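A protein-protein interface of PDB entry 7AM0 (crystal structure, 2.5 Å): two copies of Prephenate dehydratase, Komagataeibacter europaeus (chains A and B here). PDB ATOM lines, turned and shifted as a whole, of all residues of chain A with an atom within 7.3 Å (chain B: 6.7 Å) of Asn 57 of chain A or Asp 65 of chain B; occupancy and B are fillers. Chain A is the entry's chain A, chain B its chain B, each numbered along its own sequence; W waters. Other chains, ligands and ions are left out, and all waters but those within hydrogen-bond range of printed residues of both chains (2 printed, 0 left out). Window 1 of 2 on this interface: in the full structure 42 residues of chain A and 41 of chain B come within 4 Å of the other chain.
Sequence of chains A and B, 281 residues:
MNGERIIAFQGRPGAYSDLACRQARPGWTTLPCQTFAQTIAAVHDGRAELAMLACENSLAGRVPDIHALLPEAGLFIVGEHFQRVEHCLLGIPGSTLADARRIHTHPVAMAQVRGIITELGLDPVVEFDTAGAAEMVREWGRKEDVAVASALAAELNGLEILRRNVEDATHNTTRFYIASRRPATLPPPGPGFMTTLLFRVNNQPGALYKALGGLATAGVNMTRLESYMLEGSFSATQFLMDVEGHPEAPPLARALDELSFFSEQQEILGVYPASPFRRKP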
ATOM      1  N   ALA A  54      16.468  22.485  16.091  1.00  0.00           N
ATOM      2  CA  ALA A  54      16.452  21.164  15.484  1.00  0.00           C
ATOM      3  C   ALA A  54      16.447  21.339  13.968  1.00  0.00           C
ATOM      4  O   ALA A  54      15.803  22.240  13.455  1.00  0.00           O
ATOM      5  CB  ALA A  54      15.233  20.385  15.945  1.00  0.00           C
ATOM      6  N   CYS A  55      17.209  20.495  13.262  1.00  0.00           N
ATOM      7  CA  CYS A  55      17.295  20.548  11.794  1.00  0.00           C
ATOM      8  C   CYS A  55      17.067  19.202  11.089  1.00  0.00           C
ATOM      9  O   CYS A  55      16.518  19.175   9.993  1.00  0.00           O
ATOM     10  CB  CYS A  55      18.612  21.195  11.332  1.00  0.00           C
ATOM     11  SG  CYS A  55      20.114  20.273  11.722  1.00  0.00           S
ATOM     12  N   GLU A  56      17.473  18.097  11.728  1.00  0.00           N
ATOM     13  CA  GLU A  56      17.339  16.761  11.144  1.00  0.00           C
ATOM     14  C   GLU A  56      17.097  15.670  12.177  1.00  0.00           C
ATOM     15  O   GLU A  56      17.609  15.746  13.288  1.00  0.00           O
ATOM     16  CB  GLU A  56      18.606  16.397  10.364  1.00  0.00           C
ATOM     17  CG  GLU A  56      18.897  17.274   9.168  1.00  0.00           C
ATOM     18  CD  GLU A  56      20.099  16.780   8.378  1.00  0.00           C
ATOM     19  OE1 GLU A  56      19.964  15.809   7.602  1.00  0.00           O
ATOM     20  OE2 GLU A  56      21.184  17.349   8.554  1.00  0.00           O
ATOM     21  N   ASN A  57      16.346  14.642  11.759  1.00  0.00           N
ATOM     22  CA  ASN A  57      16.083  13.435  12.533  1.00  0.00           C
ATOM     23  C   ASN A  57      16.211  12.199  11.656  1.00  0.00           C
ATOM     24  O   ASN A  57      15.659  12.151  10.555  1.00  0.00           O
ATOM     25  CB  ASN A  57      14.677  13.479  13.128  1.00  0.00           C
ATOM     26  CG  ASN A  57      14.558  14.480  14.251  1.00  0.00           C
ATOM     27  OD1 ASN A  57      14.973  14.219  15.375  1.00  0.00           O
ATOM     28  ND2 ASN A  57      13.995  15.637  13.949  1.00  0.00           N
ATOM     29  N   SER A  58      16.934  11.191  12.156  1.00  0.00           N
ATOM     30  CA  SER A  58      17.190   9.961  11.411  1.00  0.00           C
ATOM     31  C   SER A  58      15.927   9.123  11.160  1.00  0.00           C
ATOM     32  O   SER A  58      15.839   8.426  10.156  1.00  0.00           O
ATOM     33  CB  SER A  58      18.266   9.124  12.113  1.00  0.00           C
ATOM     34  OG  SER A  58      17.811   8.627  13.355  1.00  0.00           O
ATOM     35  N   LEU A  59      14.957   9.199  12.079  1.00  0.00           N
ATOM     36  CA  LEU A  59      13.691   8.463  11.966  1.00  0.00           C
ATOM     37  C   LEU A  59      12.520   9.406  11.676  1.00  0.00           C
ATOM     38  O   LEU A  59      11.884   9.316  10.626  1.00  0.00           O
ATOM     39  CB  LEU A  59      13.436   7.647  13.240  1.00  0.00           C
ATOM     40  CG  LEU A  59      12.102   6.916  13.384  1.00  0.00           C
ATOM     41  CD1 LEU A  59      11.868   5.971  12.213  1.00  0.00           C
ATOM     42  CD2 LEU A  59      12.068   6.140  14.704  1.00  0.00           C
ATOM     43  N   ALA A  60      12.245  10.306  12.625  1.00  0.00           N
ATOM     44  CA  ALA A  60      11.120  11.239  12.548  1.00  0.00           C
ATOM     45  C   ALA A  60      11.269  12.335  13.587  1.00  0.00           C
ATOM     46  O   ALA A  60      12.025  12.184  14.550  1.00  0.00           O
ATOM     47  CB  ALA A  60       9.804  10.503  12.752  1.00  0.00           C
ATOM     48  N   GLY A  61      10.550  13.442  13.380  1.00  0.00           N
ATOM     49  CA  GLY A  61      10.580  14.580  14.281  1.00  0.00           C
ATOM     50  C   GLY A  61      10.001  15.845  13.674  1.00  0.00           C
ATOM     51  O   GLY A  61       9.725  15.899  12.474  1.00  0.00           O
ATOM     52  N   ARG A  62       9.799  16.857  14.525  1.00  0.00           N
ATOM     53  CA  ARG A  62       9.313  18.167  14.110  1.00  0.00           C
ATOM     54  C   ARG A  62      10.500  19.122  14.044  1.00  0.00           C
ATOM     55  O   ARG A  62      11.137  19.386  15.071  1.00  0.00           O
ATOM     56  CB  ARG A  62       8.245  18.694  15.091  1.00  0.00           C
ATOM     57  CG  ARG A  62       6.948  17.895  15.107  1.00  0.00           C
ATOM     58  CD  ARG A  62       5.778  18.679  15.712  1.00  0.00           C
ATOM     59  NE  ARG A  62       5.437  18.260  17.077  1.00  0.00           N
ATOM     60  CZ  ARG A  62       4.546  17.318  17.398  1.00  0.00           C
ATOM     61  NH1 ARG A  62       3.867  16.654  16.462  1.00  0.00           N
ATOM     62  NH2 ARG A  62       4.315  17.040  18.676  1.00  0.00           N
ATOM     63  N   VAL A  63      10.809  19.607  12.833  1.00  0.00           N
ATOM     64  CA  VAL A  63      11.885  20.563  12.612  1.00  0.00           C
ATOM     65  C   VAL A  63      11.353  21.818  11.925  1.00  0.00           C
ATOM     66  O   VAL A  63      10.509  21.735  11.037  1.00  0.00           O
ATOM     67  CB  VAL A  63      13.049  19.963  11.778  1.00  0.00           C
ATOM     68  CG1 VAL A  63      13.582  18.703  12.447  1.00  0.00           C
ATOM     69  CG2 VAL A  63      12.634  19.690  10.340  1.00  0.00           C
ATOM     70  N   GLN A  83      22.401  14.394  18.983  1.00  0.00           N
ATOM     71  CA  GLN A  83      21.833  13.804  20.186  1.00  0.00           C
ATOM     72  C   GLN A  83      21.247  12.432  19.860  1.00  0.00           C
ATOM     73  O   GLN A  83      20.333  12.315  19.047  1.00  0.00           O
ATOM     74  CB  GLN A  83      20.746  14.721  20.720  1.00  0.00           C
ATOM     75  CG  GLN A  83      20.204  14.345  22.094  1.00  0.00           C
ATOM     76  CD  GLN A  83      18.863  15.027  22.370  1.00  0.00           C
ATOM     77  OE1 GLN A  83      17.919  14.888  21.588  1.00  0.00           O
ATOM     78  NE2 GLN A  83      18.779  15.768  23.461  1.00  0.00           N
ATOM     79  N   VAL A  85      18.809  10.159  21.070  1.00  0.00           N
ATOM     80  CA  VAL A  85      17.630  10.304  21.913  1.00  0.00           C
ATOM     81  C   VAL A  85      17.494   9.085  22.822  1.00  0.00           C
ATOM     82  O   VAL A  85      17.409   7.955  22.354  1.00  0.00           O
ATOM     83  CB  VAL A  85      16.354  10.477  21.062  1.00  0.00           C
ATOM     84  CG1 VAL A  85      15.103  10.461  21.916  1.00  0.00           C
ATOM     85  CG2 VAL A  85      16.438  11.771  20.233  1.00  0.00           C
ATOM     86  N   ASN A 172      16.386   6.751  17.234  1.00  0.00           N
ATOM     87  CA  ASN A 172      16.399   8.069  16.605  1.00  0.00           C
ATOM     88  C   ASN A 172      17.573   8.920  17.086  1.00  0.00           C
ATOM     89  O   ASN A 172      17.932   8.903  18.265  1.00  0.00           O
ATOM     90  CB  ASN A 172      15.090   8.792  16.893  1.00  0.00           C
ATOM     91  CG  ASN A 172      14.952  10.100  16.114  1.00  0.00           C
ATOM     92  OD1 ASN A 172      15.118  10.131  14.893  1.00  0.00           O
ATOM     93  ND2 ASN A 172      14.650  11.182  16.815  1.00  0.00           N
ATOM     94  N   THR A 173      18.174   9.653  16.143  1.00  0.00           N
ATOM     95  CA  THR A 173      19.206  10.646  16.413  1.00  0.00           C
ATOM     96  C   THR A 173      18.691  11.974  15.893  1.00  0.00           C
ATOM     97  O   THR A 173      18.094  12.023  14.818  1.00  0.00           O
ATOM     98  CB  THR A 173      20.525  10.296  15.703  1.00  0.00           C
ATOM     99  OG1 THR A 173      20.989   9.022  16.160  1.00  0.00           O
ATOM    100  CG2 THR A 173      21.591  11.356  15.973  1.00  0.00           C
ATOM    101  N   THR A 174      18.913  13.041  16.663  1.00  0.00           N
ATOM    102  CA  THR A 174      18.476  14.374  16.292  1.00  0.00           C
ATOM    103  C   THR A 174      19.699  15.262  16.135  1.00  0.00           C
ATOM    104  O   THR A 174      20.593  15.253  16.987  1.00  0.00           O
ATOM    105  CB  THR A 174      17.530  14.971  17.349  1.00  0.00           C
ATOM    106  OG1 THR A 174      16.491  14.030  17.644  1.00  0.00           O
ATOM    107  CG2 THR A 174      16.905  16.278  16.849  1.00  0.00           C
ATOM    108  N   ARG A 175      19.739  16.012  15.026  1.00  0.00           N
ATOM    109  CA  ARG A 175      20.804  16.962  14.746  1.00  0.00           C
ATOM    110  C   ARG A 175      20.238  18.362  14.894  1.00  0.00           C
ATOM    111  O   ARG A 175      19.094  18.611  14.511  1.00  0.00           O
ATOM    112  CB  ARG A 175      21.361  16.758  13.324  1.00  0.00           C
ATOM    113  CG  ARG A 175      22.506  17.692  12.980  1.00  0.00           C
ATOM    114  CD  ARG A 175      23.016  17.501  11.567  1.00  0.00           C
ATOM    115  NE  ARG A 175      24.051  18.491  11.253  1.00  0.00           N
ATOM    116  CZ  ARG A 175      23.937  19.473  10.360  1.00  0.00           C
ATOM    117  NH1 ARG A 175      22.843  19.612   9.611  1.00  0.00           N
ATOM    118  NH2 ARG A 175      24.952  20.312  10.194  1.00  0.00           N
ATOM    119  N   PHE A 176      21.052  19.270  15.443  1.00  0.00           N
ATOM    120  CA  PHE A 176      20.651  20.652  15.691  1.00  0.00           C
ATOM    121  C   PHE A 176      21.671  21.610  15.094  1.00  0.00           C
ATOM    122  O   PHE A 176      22.863  21.320  15.099  1.00  0.00           O
ATOM    123  CB  PHE A 176      20.581  20.948  17.201  1.00  0.00           C
ATOM    124  CG  PHE A 176      19.689  20.026  17.982  1.00  0.00           C
ATOM    125  CD1 PHE A 176      20.157  18.797  18.444  1.00  0.00           C
ATOM    126  CD2 PHE A 176      18.373  20.391  18.278  1.00  0.00           C
ATOM    127  CE1 PHE A 176      19.342  17.957  19.175  1.00  0.00           C
ATOM    128  CE2 PHE A 176      17.554  19.562  19.017  1.00  0.00           C
ATOM    129  CZ  PHE A 176      18.034  18.347  19.464  1.00  0.00           C
ATOM    130  N   PHE B  36       0.459  14.727  13.278  1.00  0.00           N
ATOM    131  CA  PHE B  36       0.738  14.214  11.936  1.00  0.00           C
ATOM    132  C   PHE B  36       0.611  12.687  11.902  1.00  0.00           C
ATOM    133  O   PHE B  36       0.079  12.137  10.950  1.00  0.00           O
ATOM    134  CB  PHE B  36       2.131  14.671  11.451  1.00  0.00           C
ATOM    135  CG  PHE B  36       2.703  13.845  10.325  1.00  0.00           C
ATOM    136  CD1 PHE B  36       2.266  14.022   9.015  1.00  0.00           C
ATOM    137  CD2 PHE B  36       3.711  12.911  10.567  1.00  0.00           C
ATOM    138  CE1 PHE B  36       2.796  13.265   7.977  1.00  0.00           C
ATOM    139  CE2 PHE B  36       4.228  12.140   9.534  1.00  0.00           C
ATOM    140  CZ  PHE B  36       3.782  12.328   8.237  1.00  0.00           C
ATOM    141  N   VAL B  63       6.275  21.580   8.786  1.00  0.00           N
ATOM    142  CA  VAL B  63       6.021  20.429   7.926  1.00  0.00           C
ATOM    143  C   VAL B  63       6.569  19.152   8.556  1.00  0.00           C
ATOM    144  O   VAL B  63       7.641  19.166   9.151  1.00  0.00           O
ATOM    145  CB  VAL B  63       6.608  20.613   6.511  1.00  0.00           C
ATOM    146  CG1 VAL B  63       6.084  21.897   5.882  1.00  0.00           C
ATOM    147  CG2 VAL B  63       8.134  20.595   6.525  1.00  0.00           C
ATOM    148  N   PRO B  64       5.829  18.021   8.472  1.00  0.00           N
ATOM    149  CA  PRO B  64       6.297  16.746   9.016  1.00  0.00           C
ATOM    150  C   PRO B  64       7.396  16.102   8.168  1.00  0.00           C
ATOM    151  O   PRO B  64       7.483  16.361   6.961  1.00  0.00           O
ATOM    152  CB  PRO B  64       5.032  15.877   8.967  1.00  0.00           C
ATOM    153  CG  PRO B  64       4.249  16.447   7.833  1.00  0.00           C
ATOM    154  CD  PRO B  64       4.494  17.918   7.865  1.00  0.00           C
ATOM    155  N   ASP B  65       8.218  15.260   8.812  1.00  0.00           N
ATOM    156  CA  ASP B  65       9.222  14.446   8.148  1.00  0.00           C
ATOM    157  C   ASP B  65       8.582  13.101   7.769  1.00  0.00           C
ATOM    158  O   ASP B  65       8.396  12.224   8.618  1.00  0.00           O
ATOM    159  CB  ASP B  65      10.436  14.245   9.057  1.00  0.00           C
ATOM    160  CG  ASP B  65      11.612  13.599   8.334  1.00  0.00           C
ATOM    161  OD1 ASP B  65      11.417  13.069   7.215  1.00  0.00           O
ATOM    162  OD2 ASP B  65      12.736  13.615   8.882  1.00  0.00           O
ATOM    163  N   ILE B  66       8.259  12.957   6.478  1.00  0.00           N
ATOM    164  CA  ILE B  66       7.522  11.819   5.938  1.00  0.00           C
ATOM    165  C   ILE B  66       8.405  10.691   5.401  1.00  0.00           C
ATOM    166  O   ILE B  66       7.888   9.657   4.984  1.00  0.00           O
ATOM    167  CB  ILE B  66       6.575  12.271   4.793  1.00  0.00           C
ATOM    168  CG1 ILE B  66       7.363  12.627   3.521  1.00  0.00           C
ATOM    169  CG2 ILE B  66       5.674  13.403   5.267  1.00  0.00           C
ATOM    170  CD1 ILE B  66       6.491  13.110   2.377  1.00  0.00           C
ATOM    171  N   HIS B  67       9.726  10.887   5.421  1.00  0.00           N
ATOM    172  CA  HIS B  67      10.663  10.036   4.676  1.00  0.00           C
ATOM    173  C   HIS B  67      10.647   8.577   5.140  1.00  0.00           C
ATOM    174  O   HIS B  67      10.777   7.660   4.329  1.00  0.00           O
ATOM    175  CB  HIS B  67      12.078  10.646   4.697  1.00  0.00           C
ATOM    176  CG  HIS B  67      12.913  10.245   5.870  1.00  0.00           C
ATOM    177  ND1 HIS B  67      13.032  11.017   7.009  1.00  0.00           N
ATOM    178  CD2 HIS B  67      13.703   9.168   6.064  1.00  0.00           C
ATOM    179  CE1 HIS B  67      13.844  10.421   7.861  1.00  0.00           C
ATOM    180  NE2 HIS B  67      14.265   9.294   7.312  1.00  0.00           N
ATOM    181  N   ALA B  68      10.457   8.380   6.450  1.00  0.00           N
ATOM    182  CA  ALA B  68      10.350   7.061   7.068  1.00  0.00           C
ATOM    183  C   ALA B  68       8.897   6.695   7.363  1.00  0.00           C
ATOM    184  O   ALA B  68       8.444   5.604   7.016  1.00  0.00           O
ATOM    185  CB  ALA B  68      11.169   7.022   8.348  1.00  0.00           C
ATOM    186  N   LEU B  69       8.173   7.619   8.006  1.00  0.00           N
ATOM    187  CA  LEU B  69       6.813   7.375   8.494  1.00  0.00           C
ATOM    188  C   LEU B  69       5.783   7.045   7.411  1.00  0.00           C
ATOM    189  O   LEU B  69       4.909   6.228   7.633  1.00  0.00           O
ATOM    190  CB  LEU B  69       6.323   8.561   9.342  1.00  0.00           C
ATOM    191  CG  LEU B  69       6.936   8.689  10.746  1.00  0.00           C
ATOM    192  CD1 LEU B  69       6.433   9.963  11.413  1.00  0.00           C
ATOM    193  CD2 LEU B  69       6.621   7.494  11.636  1.00  0.00           C
ATOM    194  N   LEU B  70       5.889   7.691   6.248  1.00  0.00           N
ATOM    195  CA  LEU B  70       4.931   7.497   5.147  1.00  0.00           C
ATOM    196  C   LEU B  70       5.010   6.111   4.504  1.00  0.00           C
ATOM    197  O   LEU B  70       3.990   5.427   4.419  1.00  0.00           O
ATOM    198  CB  LEU B  70       5.053   8.601   4.089  1.00  0.00           C
ATOM    199  CG  LEU B  70       3.918   8.726   3.075  1.00  0.00           C
ATOM    200  CD1 LEU B  70       2.640   9.138   3.781  1.00  0.00           C
ATOM    201  CD2 LEU B  70       4.280   9.767   2.025  1.00  0.00           C
ATOM    202  N   GLU B 226      15.635  16.600  -1.169  1.00  0.00           N
ATOM    203  CA  GLU B 226      15.896  16.750   0.263  1.00  0.00           C
ATOM    204  C   GLU B 226      16.616  15.541   0.856  1.00  0.00           C
ATOM    205  O   GLU B 226      16.139  14.396   0.735  1.00  0.00           O
ATOM    206  CB  GLU B 226      14.571  16.955   1.002  1.00  0.00           C
ATOM    207  CG  GLU B 226      14.725  17.252   2.488  1.00  0.00           C
ATOM    208  CD  GLU B 226      13.437  17.739   3.118  1.00  0.00           C
ATOM    209  OE1 GLU B 226      12.798  18.656   2.572  1.00  0.00           O
ATOM    210  OE2 GLU B 226      13.057  17.198   4.172  1.00  0.00           O
ATOM    211  N   TYR B 228      18.467  13.252   4.030  1.00  0.00           N
ATOM    212  CA  TYR B 228      18.209  12.777   5.374  1.00  0.00           C
ATOM    213  C   TYR B 228      19.388  11.960   5.893  1.00  0.00           C
ATOM    214  O   TYR B 228      20.029  11.226   5.127  1.00  0.00           O
ATOM    215  CB  TYR B 228      16.959  11.897   5.402  1.00  0.00           C
ATOM    216  CG  TYR B 228      15.707  12.618   4.954  1.00  0.00           C
ATOM    217  CD1 TYR B 228      14.978  13.430   5.834  1.00  0.00           C
ATOM    218  CD2 TYR B 228      15.269  12.511   3.643  1.00  0.00           C
ATOM    219  CE1 TYR B 228      13.847  14.109   5.405  1.00  0.00           C
ATOM    220  CE2 TYR B 228      14.141  13.179   3.209  1.00  0.00           C
ATOM    221  CZ  TYR B 228      13.435  13.972   4.088  1.00  0.00           C
ATOM    222  OH  TYR B 228      12.312  14.621   3.639  1.00  0.00           O
ATOM    223  N   MET B 229      19.655  12.076   7.201  1.00  0.00           N
ATOM    224  CA  MET B 229      20.638  11.251   7.887  1.00  0.00           C
ATOM    225  C   MET B 229      20.130   9.821   8.011  1.00  0.00           C
ATOM    226  O   MET B 229      18.909   9.584   8.082  1.00  0.00           O
ATOM    227  CB  MET B 229      20.873  11.751   9.323  1.00  0.00           C
ATOM    228  CG  MET B 229      21.242  13.200   9.506  1.00  0.00           C
ATOM    229  SD  MET B 229      21.524  13.444  11.286  1.00  0.00           S
ATOM    230  CE  MET B 229      19.850  13.208  11.858  1.00  0.00           C
ATOM    231  N   GLU B 231      20.345   6.490  10.533  1.00  0.00           N
ATOM    232  CA  GLU B 231      20.548   6.199  11.945  1.00  0.00           C
ATOM    233  C   GLU B 231      21.843   5.406  12.136  1.00  0.00           C
ATOM    234  O   GLU B 231      22.008   4.328  11.564  1.00  0.00           O
ATOM    235  CB  GLU B 231      19.340   5.448  12.525  1.00  0.00           C
ATOM    236  CG  GLU B 231      19.470   5.019  13.984  1.00  0.00           C
ATOM    237  CD  GLU B 231      19.925   6.134  14.920  1.00  0.00           C
ATOM    238  OE1 GLU B 231      19.493   7.296  14.750  1.00  0.00           O
ATOM    239  OE2 GLU B 231      20.719   5.842  15.840  1.00  0.00           O
HETATM  240  O   HOH W   1       8.190  14.136  11.555  1.00  0.00           O
HETATM  241  O   HOH W   2      12.534  15.443  11.367  1.00  0.00           O
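Of chain B, only Asp 65 (3.7 Å), His 67 (3.7 Å) and Met 229 (3.8 Å) come within 4 Å of Asn 57 of chain A. Of the printed residues of chain B, Asn 172 of chain A touches Glu 231. Of the printed residues of chain A, Met 229 of chain B touches Glu 56, Asn 57, Ser 58, Thr 173 and Arg 175. The nearest residue of chain B that does not touch Asn 57 of chain A is Tyr 228 of chain B (4.9 Å). The nearest residue of chain A that does not touch Asp 65 of chain B is Ala 60 of chain A (4.7 Å).
OG of Ser 58 of chain A lies within hydrogen-bond range of OE1 of Glu 231 of chain B (2.6 Å). O of Ser 58 of chain A lies within hydrogen-bond range of NE2 of His 67 of chain B. The side-chain hydroxyl of Thr 173 of chain A is in hydrogen-bond range of the side-chain carboxylate of Glu 231 of chain B.
Position printed for both chains: 63.
Of the 13 printed residues of chain B, 6 touch a printed residue of chain A. Hydrophobic or aromatic side chains of chain B that line the printed part of chain A: His 67, Ala 68, Leu 69 and Met 229. Along chain B the printed residues that touch a printed residue of chain A span positions 65 to 231. Printed residues of chain A that touch a printed residue of chain B: Glu 56, Asn 57, Ser 58, Leu 59, Ala 60, Gly 61, Asn 172, Thr 173 and Arg 175. Along chain A the printed residues that touch a printed residue of chain B span positions 56 to 175.
CG of Met 229 of chain B touches OE1 of Glu 56 of chain A, at 3.5 Å. Asn 57 of chain A touches Met 229 of chain B. N of Ser 58 of chain A touches CE of Met 229 of chain B, 3.6 Å away. O of Leu 59 of chain A touches CE1 of His 67 of chain B (3.6 Å). CB of Ala 68 of chain B touches O of Leu 59 of chain A, 3.3 Å away. Ala 60 of chain A touches Leu 69 of chain B (CB to CD1, 3.7 Å). Gly 61 of chain A touches Asp 65 of chain B (O to CB, 3.9 Å). Asn 172 of chain A touches Glu 231 of chain B (C to OE1, 3.4 Å). CE of Met 229 of chain B touches O of Thr 173 of chain A, at 3.6 Å. CB of Arg 175 of chain A touches SD of Met 229 of chain B (3.9 Å).
Water W1 lies within hydrogen-bond range of the backbone carbonyl oxygen of Gly 61 of chain A and the backbone NH of Asp 65 of chain B. Water W2 lies within hydrogen-bond range of ND2 of Asn 57 of chain A (3.0 Å), O of Gly 61 of chain A (3.1 Å) and OD2 of Asp 65 of chain B (3.1 Å).
OD1 of Asn 57 of chain A is in hydrogen-bond range of OG1 of Thr 174 of chain A, 2.7 Å away. The backbone NH (N) of Leu 59 of chain A sits at hydrogen-bond distance from the side-chain amide oxygen (OD1) of Asn 172 of chain A (3.0 Å). The side-chain hydroxyl (OG) of Ser 58 of chain A is in hydrogen-bond range of the backbone NH (N) of Thr 173 of chain A, at 3.0 Å. The side-chain amide nitrogen (ND2) of Asn 172 of chain A sits at hydrogen-bond distance from the side-chain hydroxyl (OG1) of Thr 174 of chain A, 3.5 Å away. The backbone NH of Cys 55 of chain A is in hydrogen-bond range of the backbone carbonyl oxygen of Arg 175 of chain A. ND1 of His 67 of chain B lies within hydrogen-bond range of OD1 of Asp 65 of chain B (2.6 Å).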
